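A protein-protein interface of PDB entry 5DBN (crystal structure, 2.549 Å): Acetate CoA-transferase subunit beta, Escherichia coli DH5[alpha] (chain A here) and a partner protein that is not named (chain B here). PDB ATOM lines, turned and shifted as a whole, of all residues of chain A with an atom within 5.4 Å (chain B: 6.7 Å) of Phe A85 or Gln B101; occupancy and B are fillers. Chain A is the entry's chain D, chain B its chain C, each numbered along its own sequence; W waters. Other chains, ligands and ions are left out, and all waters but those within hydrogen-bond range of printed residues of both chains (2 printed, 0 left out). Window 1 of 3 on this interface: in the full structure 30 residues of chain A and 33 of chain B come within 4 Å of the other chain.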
ATOM      1  N   GLN A  44      31.317  -2.117  29.086  1.00  0.00           N
ATOM      2  CA  GLN A  44      31.741  -3.336  28.401  1.00  0.00           C
ATOM      3  C   GLN A  44      31.783  -3.104  26.895  1.00  0.00           C
ATOM      4  O   GLN A  44      30.866  -2.514  26.328  1.00  0.00           O
ATOM      5  CB  GLN A  44      30.795  -4.492  28.748  1.00  0.00           C
ATOM      6  CG  GLN A  44      31.329  -5.882  28.407  1.00  0.00           C
ATOM      7  CD  GLN A  44      30.971  -6.348  27.005  1.00  0.00           C
ATOM      8  OE1 GLN A  44      30.378  -5.613  26.217  1.00  0.00           O
ATOM      9  NE2 GLN A  44      31.332  -7.589  26.692  1.00  0.00           N
ATOM     10  N   GLU A  46      31.992  -4.910  23.179  1.00  0.00           N
ATOM     11  CA  GLU A  46      31.664  -6.193  22.550  1.00  0.00           C
ATOM     12  C   GLU A  46      32.895  -6.903  22.007  1.00  0.00           C
ATOM     13  O   GLU A  46      32.992  -8.127  22.074  1.00  0.00           O
ATOM     14  CB  GLU A  46      30.660  -5.999  21.409  1.00  0.00           C
ATOM     15  CG  GLU A  46      29.341  -5.387  21.830  1.00  0.00           C
ATOM     16  CD  GLU A  46      29.336  -3.878  21.710  1.00  0.00           C
ATOM     17  OE1 GLU A  46      30.065  -3.217  22.479  1.00  0.00           O
ATOM     18  OE2 GLU A  46      28.605  -3.354  20.844  1.00  0.00           O
ATOM     19  N   ASN A  47      33.831  -6.131  21.467  1.00  0.00           N
ATOM     20  CA  ASN A  47      35.033  -6.703  20.876  1.00  0.00           C
ATOM     21  C   ASN A  47      35.933  -7.355  21.926  1.00  0.00           C
ATOM     22  O   ASN A  47      36.957  -7.950  21.585  1.00  0.00           O
ATOM     23  CB  ASN A  47      35.807  -5.638  20.088  1.00  0.00           C
ATOM     24  CG  ASN A  47      36.000  -4.353  20.866  1.00  0.00           C
ATOM     25  OD1 ASN A  47      35.186  -4.002  21.719  1.00  0.00           O
ATOM     26  ND2 ASN A  47      37.076  -3.636  20.566  1.00  0.00           N
ATOM     27  N   ASP A  80      38.292 -12.964  25.088  1.00  0.00           N
ATOM     28  CA  ASP A  80      37.876 -13.259  23.717  1.00  0.00           C
ATOM     29  C   ASP A  80      36.377 -13.021  23.526  1.00  0.00           C
ATOM     30  O   ASP A  80      35.667 -12.677  24.469  1.00  0.00           O
ATOM     31  CB  ASP A  80      38.249 -14.702  23.341  1.00  0.00           C
ATOM     32  CG  ASP A  80      37.586 -15.745  24.233  1.00  0.00           C
ATOM     33  OD1 ASP A  80      36.361 -15.667  24.469  1.00  0.00           O
ATOM     34  OD2 ASP A  80      38.301 -16.659  24.699  1.00  0.00           O
ATOM     35  N   SER A  81      35.908 -13.208  22.297  1.00  0.00           N
ATOM     36  CA  SER A  81      34.527 -12.893  21.944  1.00  0.00           C
ATOM     37  C   SER A  81      33.536 -13.878  22.559  1.00  0.00           C
ATOM     38  O   SER A  81      32.400 -13.517  22.857  1.00  0.00           O
ATOM     39  CB  SER A  81      34.364 -12.863  20.425  1.00  0.00           C
ATOM     40  OG  SER A  81      35.233 -11.902  19.845  1.00  0.00           O
ATOM     41  N   ALA A  82      33.961 -15.126  22.726  1.00  0.00           N
ATOM     42  CA  ALA A  82      33.113 -16.135  23.354  1.00  0.00           C
ATOM     43  C   ALA A  82      32.803 -15.742  24.794  1.00  0.00           C
ATOM     44  O   ALA A  82      31.661 -15.833  25.238  1.00  0.00           O
ATOM     45  CB  ALA A  82      33.778 -17.501  23.305  1.00  0.00           C
ATOM     46  N   MET A  83      33.836 -15.327  25.522  1.00  0.00           N
ATOM     47  CA  MET A  83      33.682 -14.824  26.882  1.00  0.00           C
ATOM     48  C   MET A  83      32.825 -13.564  26.886  1.00  0.00           C
ATOM     49  O   MET A  83      31.959 -13.390  27.744  1.00  0.00           O
ATOM     50  CB  MET A  83      35.049 -14.532  27.503  1.00  0.00           C
ATOM     51  CG  MET A  83      34.997 -13.953  28.915  1.00  0.00           C
ATOM     52  SD  MET A  83      34.141 -15.016  30.092  1.00  0.00           S
ATOM     53  CE  MET A  83      34.420 -14.114  31.613  1.00  0.00           C
ATOM     54  N   SER A  84      33.087 -12.686  25.922  1.00  0.00           N
ATOM     55  CA  SER A  84      32.362 -11.427  25.802  1.00  0.00           C
ATOM     56  C   SER A  84      30.858 -11.649  25.707  1.00  0.00           C
ATOM     57  O   SER A  84      30.084 -11.031  26.436  1.00  0.00           O
ATOM     58  CB  SER A  84      32.847 -10.646  24.579  1.00  0.00           C
ATOM     59  OG  SER A  84      32.167  -9.410  24.469  1.00  0.00           O
ATOM     60  N   PHE A  85      30.442 -12.515  24.792  1.00  0.00           N
ATOM     61  CA  PHE A  85      29.022 -12.766  24.597  1.00  0.00           C
ATOM     62  C   PHE A  85      28.489 -13.832  25.555  1.00  0.00           C
ATOM     63  O   PHE A  85      27.282 -14.038  25.648  1.00  0.00           O
ATOM     64  CB  PHE A  85      28.757 -13.127  23.140  1.00  0.00           C
ATOM     65  CG  PHE A  85      28.792 -11.931  22.235  1.00  0.00           C
ATOM     66  CD1 PHE A  85      29.984 -11.501  21.681  1.00  0.00           C
ATOM     67  CD2 PHE A  85      27.643 -11.199  21.990  1.00  0.00           C
ATOM     68  CE1 PHE A  85      30.024 -10.388  20.869  1.00  0.00           C
ATOM     69  CE2 PHE A  85      27.676 -10.083  21.179  1.00  0.00           C
ATOM     70  CZ  PHE A  85      28.870  -9.676  20.620  1.00  0.00           C
ATOM     71  N   ALA A  86      29.389 -14.517  26.253  1.00  0.00           N
ATOM     72  CA  ALA A  86      28.997 -15.301  27.418  1.00  0.00           C
ATOM     73  C   ALA A  86      28.542 -14.347  28.521  1.00  0.00           C
ATOM     74  O   ALA A  86      27.551 -14.596  29.208  1.00  0.00           O
ATOM     75  CB  ALA A  86      30.142 -16.180  27.900  1.00  0.00           C
ATOM     76  N   LEU A  87      29.290 -13.260  28.692  1.00  0.00           N
ATOM     77  CA  LEU A  87      28.921 -12.211  29.636  1.00  0.00           C
ATOM     78  C   LEU A  87      27.624 -11.530  29.209  1.00  0.00           C
ATOM     79  O   LEU A  87      26.699 -11.378  30.007  1.00  0.00           O
ATOM     80  CB  LEU A  87      30.037 -11.166  29.755  1.00  0.00           C
ATOM     81  CG  LEU A  87      31.362 -11.570  30.406  1.00  0.00           C
ATOM     82  CD1 LEU A  87      32.422 -10.515  30.139  1.00  0.00           C
ATOM     83  CD2 LEU A  87      31.189 -11.787  31.902  1.00  0.00           C
ATOM     84  N   ILE A  88      27.571 -11.108  27.948  1.00  0.00           N
ATOM     85  CA  ILE A  88      26.412 -10.394  27.419  1.00  0.00           C
ATOM     86  C   ILE A  88      25.150 -11.253  27.444  1.00  0.00           C
ATOM     87  O   ILE A  88      24.095 -10.804  27.890  1.00  0.00           O
ATOM     88  CB  ILE A  88      26.671  -9.905  25.972  1.00  0.00           C
ATOM     89  CG1 ILE A  88      27.738  -8.806  25.967  1.00  0.00           C
ATOM     90  CG2 ILE A  88      25.384  -9.392  25.323  1.00  0.00           C
ATOM     91  CD1 ILE A  88      28.245  -8.426  24.588  1.00  0.00           C
ATOM     92  N   ARG A  89      25.262 -12.489  26.970  1.00  0.00           N
ATOM     93  CA  ARG A  89      24.101 -13.361  26.841  1.00  0.00           C
ATOM     94  C   ARG A  89      23.737 -14.002  28.180  1.00  0.00           C
ATOM     95  O   ARG A  89      22.582 -14.359  28.412  1.00  0.00           O
ATOM     96  CB  ARG A  89      24.371 -14.436  25.781  1.00  0.00           C
ATOM     97  CG  ARG A  89      23.154 -15.254  25.373  1.00  0.00           C
ATOM     98  CD  ARG A  89      23.478 -16.242  24.250  1.00  0.00           C
ATOM     99  NE  ARG A  89      24.743 -16.941  24.483  1.00  0.00           N
ATOM    100  CZ  ARG A  89      25.851 -16.794  23.758  1.00  0.00           C
ATOM    101  NH1 ARG A  89      25.893 -15.980  22.711  1.00  0.00           N
ATOM    102  NH2 ARG A  89      26.936 -17.479  24.083  1.00  0.00           N
ATOM    103  N   GLY A  90      24.723 -14.131  29.062  1.00  0.00           N
ATOM    104  CA  GLY A  90      24.531 -14.815  30.329  1.00  0.00           C
ATOM    105  C   GLY A  90      23.906 -13.949  31.409  1.00  0.00           C
ATOM    106  O   GLY A  90      23.684 -14.412  32.528  1.00  0.00           O
ATOM    107  N   MET A 122      23.515  -7.133  12.095  1.00  0.00           N
ATOM    108  CA  MET A 122      22.978  -6.907  13.436  1.00  0.00           C
ATOM    109  C   MET A 122      24.068  -6.737  14.487  1.00  0.00           C
ATOM    110  O   MET A 122      23.826  -6.161  15.548  1.00  0.00           O
ATOM    111  CB  MET A 122      22.045  -8.055  13.843  1.00  0.00           C
ATOM    112  CG  MET A 122      22.700  -9.431  13.949  1.00  0.00           C
ATOM    113  SD  MET A 122      23.056 -10.204  12.360  1.00  0.00           S
ATOM    114  CE  MET A 122      21.403 -10.474  11.722  1.00  0.00           C
ATOM    115  N   GLY A 123      25.262  -7.240  14.196  1.00  0.00           N
ATOM    116  CA  GLY A 123      26.355  -7.192  15.150  1.00  0.00           C
ATOM    117  C   GLY A 123      26.021  -7.934  16.432  1.00  0.00           C
ATOM    118  O   GLY A 123      25.647  -9.106  16.394  1.00  0.00           O
ATOM    119  N   GLY A 124      26.132  -7.240  17.564  1.00  0.00           N
ATOM    120  CA  GLY A 124      25.864  -7.830  18.865  1.00  0.00           C
ATOM    121  C   GLY A 124      24.590  -7.323  19.517  1.00  0.00           C
ATOM    122  O   GLY A 124      24.362  -7.552  20.706  1.00  0.00           O
ATOM    123  N   ASP A 127      22.036 -10.220  20.814  1.00  0.00           N
ATOM    124  CA  ASP A 127      22.542 -10.797  22.057  1.00  0.00           C
ATOM    125  C   ASP A 127      22.375  -9.819  23.219  1.00  0.00           C
ATOM    126  O   ASP A 127      21.980 -10.205  24.319  1.00  0.00           O
ATOM    127  CB  ASP A 127      24.016 -11.185  21.913  1.00  0.00           C
ATOM    128  CG  ASP A 127      24.236 -12.296  20.903  1.00  0.00           C
ATOM    129  OD1 ASP A 127      24.022 -13.476  21.255  1.00  0.00           O
ATOM    130  OD2 ASP A 127      24.622 -11.987  19.757  1.00  0.00           O
ATOM    131  N   PHE B  27      38.762  -8.058  14.815  1.00  0.00           N
ATOM    132  CA  PHE B  27      37.529  -7.297  14.973  1.00  0.00           C
ATOM    133  C   PHE B  27      37.715  -5.926  14.329  1.00  0.00           C
ATOM    134  O   PHE B  27      38.516  -5.117  14.800  1.00  0.00           O
ATOM    135  CB  PHE B  27      37.159  -7.165  16.453  1.00  0.00           C
ATOM    136  CG  PHE B  27      35.831  -6.501  16.692  1.00  0.00           C
ATOM    137  CD1 PHE B  27      35.705  -5.123  16.622  1.00  0.00           C
ATOM    138  CD2 PHE B  27      34.708  -7.255  16.987  1.00  0.00           C
ATOM    139  CE1 PHE B  27      34.488  -4.511  16.842  1.00  0.00           C
ATOM    140  CE2 PHE B  27      33.485  -6.649  17.207  1.00  0.00           C
ATOM    141  CZ  PHE B  27      33.376  -5.274  17.134  1.00  0.00           C
ATOM    142  N   ASN B  53      34.411 -11.981  12.027  1.00  0.00           N
ATOM    143  CA  ASN B  53      33.425 -11.187  12.748  1.00  0.00           C
ATOM    144  C   ASN B  53      32.766 -10.166  11.836  1.00  0.00           C
ATOM    145  O   ASN B  53      31.583  -9.858  11.978  1.00  0.00           O
ATOM    146  CB  ASN B  53      34.063 -10.478  13.938  1.00  0.00           C
ATOM    147  CG  ASN B  53      33.066  -9.633  14.704  1.00  0.00           C
ATOM    148  OD1 ASN B  53      32.379 -10.124  15.598  1.00  0.00           O
ATOM    149  ND2 ASN B  53      32.974  -8.357  14.349  1.00  0.00           N
ATOM    150  N   ALA B  76      29.427 -13.638   8.533  1.00  0.00           N
ATOM    151  CA  ALA B  76      29.841 -12.613   9.486  1.00  0.00           C
ATOM    152  C   ALA B  76      28.636 -12.012  10.198  1.00  0.00           C
ATOM    153  O   ALA B  76      27.505 -12.440   9.980  1.00  0.00           O
ATOM    154  CB  ALA B  76      30.628 -11.531   8.780  1.00  0.00           C
ATOM    155  N   SER B  77      28.893 -11.022  11.051  1.00  0.00           N
ATOM    156  CA  SER B  77      27.844 -10.387  11.842  1.00  0.00           C
ATOM    157  C   SER B  77      27.606  -8.936  11.441  1.00  0.00           C
ATOM    158  O   SER B  77      26.544  -8.380  11.725  1.00  0.00           O
ATOM    159  CB  SER B  77      28.193 -10.450  13.332  1.00  0.00           C
ATOM    160  OG  SER B  77      29.304  -9.622  13.635  1.00  0.00           O
ATOM    161  N   HIS B  78      28.593  -8.321  10.794  1.00  0.00           N
ATOM    162  CA  HIS B  78      28.485  -6.918  10.403  1.00  0.00           C
ATOM    163  C   HIS B  78      29.296  -6.619   9.146  1.00  0.00           C
ATOM    164  O   HIS B  78      30.407  -7.123   8.982  1.00  0.00           O
ATOM    165  CB  HIS B  78      28.940  -6.017  11.550  1.00  0.00           C
ATOM    166  CG  HIS B  78      28.409  -4.621  11.465  1.00  0.00           C
ATOM    167  ND1 HIS B  78      29.081  -3.606  10.818  1.00  0.00           N
ATOM    168  CD2 HIS B  78      27.267  -4.072  11.943  1.00  0.00           C
ATOM    169  CE1 HIS B  78      28.376  -2.491  10.903  1.00  0.00           C
ATOM    170  NE2 HIS B  78      27.271  -2.747  11.581  1.00  0.00           N
ATOM    171  N   VAL B  99      25.026 -13.334  10.714  1.00  0.00           N
ATOM    172  CA  VAL B  99      24.728 -14.092  11.925  1.00  0.00           C
ATOM    173  C   VAL B  99      24.964 -13.213  13.150  1.00  0.00           C
ATOM    174  O   VAL B  99      25.930 -12.453  13.183  1.00  0.00           O
ATOM    175  CB  VAL B  99      25.604 -15.359  12.025  1.00  0.00           C
ATOM    176  CG1 VAL B  99      25.246 -16.169  13.270  1.00  0.00           C
ATOM    177  CG2 VAL B  99      25.453 -16.210  10.773  1.00  0.00           C
ATOM    178  N   PRO B 100      24.079 -13.300  14.159  1.00  0.00           N
ATOM    179  CA  PRO B 100      24.367 -12.580  15.404  1.00  0.00           C
ATOM    180  C   PRO B 100      25.745 -12.934  15.951  1.00  0.00           C
ATOM    181  O   PRO B 100      26.133 -14.104  15.956  1.00  0.00           O
ATOM    182  CB  PRO B 100      23.253 -13.046  16.342  1.00  0.00           C
ATOM    183  CG  PRO B 100      22.121 -13.365  15.435  1.00  0.00           C
ATOM    184  CD  PRO B 100      22.743 -13.922  14.184  1.00  0.00           C
ATOM    185  N   GLN B 101      26.482 -11.913  16.373  1.00  0.00           N
ATOM    186  CA  GLN B 101      27.872 -12.068  16.788  1.00  0.00           C
ATOM    187  C   GLN B 101      28.043 -13.144  17.858  1.00  0.00           C
ATOM    188  O   GLN B 101      28.902 -14.017  17.737  1.00  0.00           O
ATOM    189  CB  GLN B 101      28.409 -10.735  17.298  1.00  0.00           C
ATOM    190  CG  GLN B 101      29.925 -10.686  17.402  1.00  0.00           C
ATOM    191  CD  GLN B 101      30.461  -9.298  17.721  1.00  0.00           C
ATOM    192  OE1 GLN B 101      31.452  -9.159  18.437  1.00  0.00           O
ATOM    193  NE2 GLN B 101      29.820  -8.268  17.177  1.00  0.00           N
ATOM    194  N   GLY B 102      27.239 -13.060  18.911  1.00  0.00           N
ATOM    195  CA  GLY B 102      27.275 -14.042  19.979  1.00  0.00           C
ATOM    196  C   GLY B 102      26.981 -15.453  19.503  1.00  0.00           C
ATOM    197  O   GLY B 102      27.516 -16.418  20.044  1.00  0.00           O
ATOM    198  N   THR B 103      26.132 -15.576  18.487  1.00  0.00           N
ATOM    199  CA  THR B 103      25.811 -16.882  17.916  1.00  0.00           C
ATOM    200  C   THR B 103      26.972 -17.393  17.079  1.00  0.00           C
ATOM    201  O   THR B 103      27.382 -18.547  17.209  1.00  0.00           O
ATOM    202  CB  THR B 103      24.538 -16.834  17.042  1.00  0.00           C
ATOM    203  OG1 THR B 103      23.407 -16.489  17.850  1.00  0.00           O
ATOM    204  CG2 THR B 103      24.286 -18.182  16.380  1.00  0.00           C
ATOM    205  N   LEU B 104      27.493 -16.524  16.219  1.00  0.00           N
ATOM    206  CA  LEU B 104      28.593 -16.878  15.332  1.00  0.00           C
ATOM    207  C   LEU B 104      29.796 -17.404  16.113  1.00  0.00           C
ATOM    208  O   LEU B 104      30.351 -18.449  15.773  1.00  0.00           O
ATOM    209  CB  LEU B 104      28.996 -15.669  14.486  1.00  0.00           C
ATOM    210  CG  LEU B 104      30.109 -15.892  13.458  1.00  0.00           C
ATOM    211  CD1 LEU B 104      29.722 -16.935  12.420  1.00  0.00           C
ATOM    212  CD2 LEU B 104      30.433 -14.569  12.779  1.00  0.00           C
ATOM    213  N   ILE B 105      30.206 -16.674  17.145  1.00  0.00           N
ATOM    214  CA  ILE B 105      31.358 -17.080  17.940  1.00  0.00           C
ATOM    215  C   ILE B 105      31.103 -18.419  18.643  1.00  0.00           C
ATOM    216  O   ILE B 105      32.018 -19.227  18.800  1.00  0.00           O
ATOM    217  CB  ILE B 105      31.745 -15.993  18.977  1.00  0.00           C
ATOM    218  CG1 ILE B 105      33.119 -16.291  19.585  1.00  0.00           C
ATOM    219  CG2 ILE B 105      30.685 -15.854  20.068  1.00  0.00           C
ATOM    220  CD1 ILE B 105      34.266 -16.205  18.588  1.00  0.00           C
ATOM    221  N   GLU B 106      29.862 -18.653  19.063  1.00  0.00           N
ATOM    222  CA  GLU B 106      29.510 -19.922  19.700  1.00  0.00           C
ATOM    223  C   GLU B 106      29.479 -21.066  18.689  1.00  0.00           C
ATOM    224  O   GLU B 106      29.783 -22.209  19.031  1.00  0.00           O
ATOM    225  CB  GLU B 106      28.159 -19.820  20.411  1.00  0.00           C
ATOM    226  CG  GLU B 106      28.231 -19.207  21.797  1.00  0.00           C
ATOM    227  CD  GLU B 106      29.093 -20.019  22.750  1.00  0.00           C
ATOM    228  OE1 GLU B 106      29.073 -21.266  22.658  1.00  0.00           O
ATOM    229  OE2 GLU B 106      29.800 -19.413  23.582  1.00  0.00           O
ATOM    230  N   THR B 122      18.939 -15.799  21.173  1.00  0.00           N
ATOM    231  CA  THR B 122      19.235 -14.730  20.231  1.00  0.00           C
ATOM    232  C   THR B 122      18.715 -15.072  18.841  1.00  0.00           C
ATOM    233  O   THR B 122      19.029 -16.125  18.288  1.00  0.00           O
ATOM    234  CB  THR B 122      20.750 -14.458  20.166  1.00  0.00           C
ATOM    235  OG1 THR B 122      21.245 -14.209  21.486  1.00  0.00           O
ATOM    236  CG2 THR B 122      21.050 -13.258  19.280  1.00  0.00           C
ATOM    237  N   PHE B 175      38.328 -12.988  18.003  1.00  0.00           N
ATOM    238  CA  PHE B 175      38.019 -14.280  17.394  1.00  0.00           C
ATOM    239  C   PHE B 175      39.212 -15.235  17.347  1.00  0.00           C
ATOM    240  O   PHE B 175      39.029 -16.446  17.215  1.00  0.00           O
ATOM    241  CB  PHE B 175      37.488 -14.073  15.967  1.00  0.00           C
ATOM    242  CG  PHE B 175      35.991 -13.938  15.880  1.00  0.00           C
ATOM    243  CD1 PHE B 175      35.299 -13.111  16.747  1.00  0.00           C
ATOM    244  CD2 PHE B 175      35.279 -14.627  14.911  1.00  0.00           C
ATOM    245  CE1 PHE B 175      33.923 -12.984  16.661  1.00  0.00           C
ATOM    246  CE2 PHE B 175      33.902 -14.504  14.819  1.00  0.00           C
ATOM    247  CZ  PHE B 175      33.225 -13.681  15.694  1.00  0.00           C
HETATM  248  O   HOH W   1      33.721  -9.799  19.619  1.00  0.00           O
HETATM  249  O   HOH W   2      23.632 -15.972  20.568  1.00  0.00           O
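Water W1 lies within hydrogen-bond range of OG of Ser A81 (2.6 Å), OE1 of Gln B101 (2.6 Å) and O of Glu A46 (3.1 Å).
Water W2 lies within hydrogen-bond range of OD1 of Asp A127, OG1 of Thr B103, OG1 of Thr B122 and NH1 of Arg A89.
Among the printed residues, pairs that only touch across the chains: Phe A85 with Gln B101, Ser A81 with Phe B175, Phe A85 with Gly B102, Ala A82 with Ile B105, Asn A47 with Phe B27, Ser A81 with Ile B105, Asp A127 with Pro B100, Gly A123 with Pro B100, Gly A124 with Gln B101 and Asp A127 with Gln B101.
O of Ser B77 is in hydrogen-bond range of N of Met A122, at 3.3 Å.
The backbone NH (N) of Gly A123 sits at hydrogen-bond distance from the backbone carbonyl oxygen (O) of Ser B77 (3.0 Å).
N of Gln B101 sits at hydrogen-bond distance from O of Gly A123 (2.9 Å).
O of Gly B102 lies within hydrogen-bond range of NH1 of Arg A89.
The side-chain carboxylate of Asp A127 sits at hydrogen-bond distance from the backbone NH of Gly B102 (3.0 Å).
The side-chain carboxylate (OE2) of Glu B106 is in salt-bridge range of the guanidinium group (NH2) of Arg A89, 3.5 Å away.
OG1 of Thr B122 is in hydrogen-bond range of OD1 of Asp A127.
The side-chain sulfur of Met A122 sits close to the backbone carbonyl oxygen of Val B99.
N of Pro B100 sits close to SD of Met A122 (3.7 Å).
Hydrophobic or aromatic side chains of chain A that line the printed part of chain B: Ala A82, Phe A85 and Met A122.
Of the 15 printed residues of chain B, 10 touch a printed residue of chain A.
Printed residues of chain B that touch a printed residue of chain A: Phe B27, Ser B77, Val B99, Pro B100, Gln B101, Gly B102, Ile B105, Glu B106, Thr B122 and Phe B175.
Hydrophobic or aromatic side chains of chain B that line the printed part of chain A: Phe B27, Pro B100, Ile B105 and Phe B175.
Along chain B the printed residues that touch a printed residue of chain A span positions 27 to 175.
Among the printed residues, 19 pairs touch across the chains.
Among the printed residues, Asp or Glu carboxylates within 4 Å of a Lys or Arg side-chain nitrogen of the other chain: Arg A89 with Glu B106.
OG of Ser B77 lies within hydrogen-bond range of O of Asn B53, at 2.8 Å.
The side-chain amide oxygen of Gln B101 lies close to the side-chain amide oxygen of Asn B53.
The backbone carbonyl oxygen of Ala B76 lies within hydrogen-bond range of the backbone NH of Val B99 (2.7 Å).
N of Ala A82 lies within hydrogen-bond range of OD1 of Asp A80.
The side-chain carboxylate (OD1) of Asp A127 lies within salt-bridge range of the guanidinium group (NH1) of Arg A89 (3.4 Å).
Of chain B, only Gln B101 and Gly B102 come within 4 Å of Phe A85.
Of chain A, only Phe A85, Gly A123, Gly A124 and Asp A127 come within 4 Å of Gln B101.
Of the printed residues of chain A, Thr B122 touches Asp A127.
Of the printed residues of chain B, Arg A89 touches Gly B102 (3.2 Å) and Glu B106 (3.1 Å).
Of the printed residues of chain A, Val B99 touches Met A122.
Met A83 touches none of the printed residues of chain B.
Gln A44 touches none of the printed residues of chain B.
The nearest residue of chain B that does not touch Phe A85 is Ile B105 (4.5 Å).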
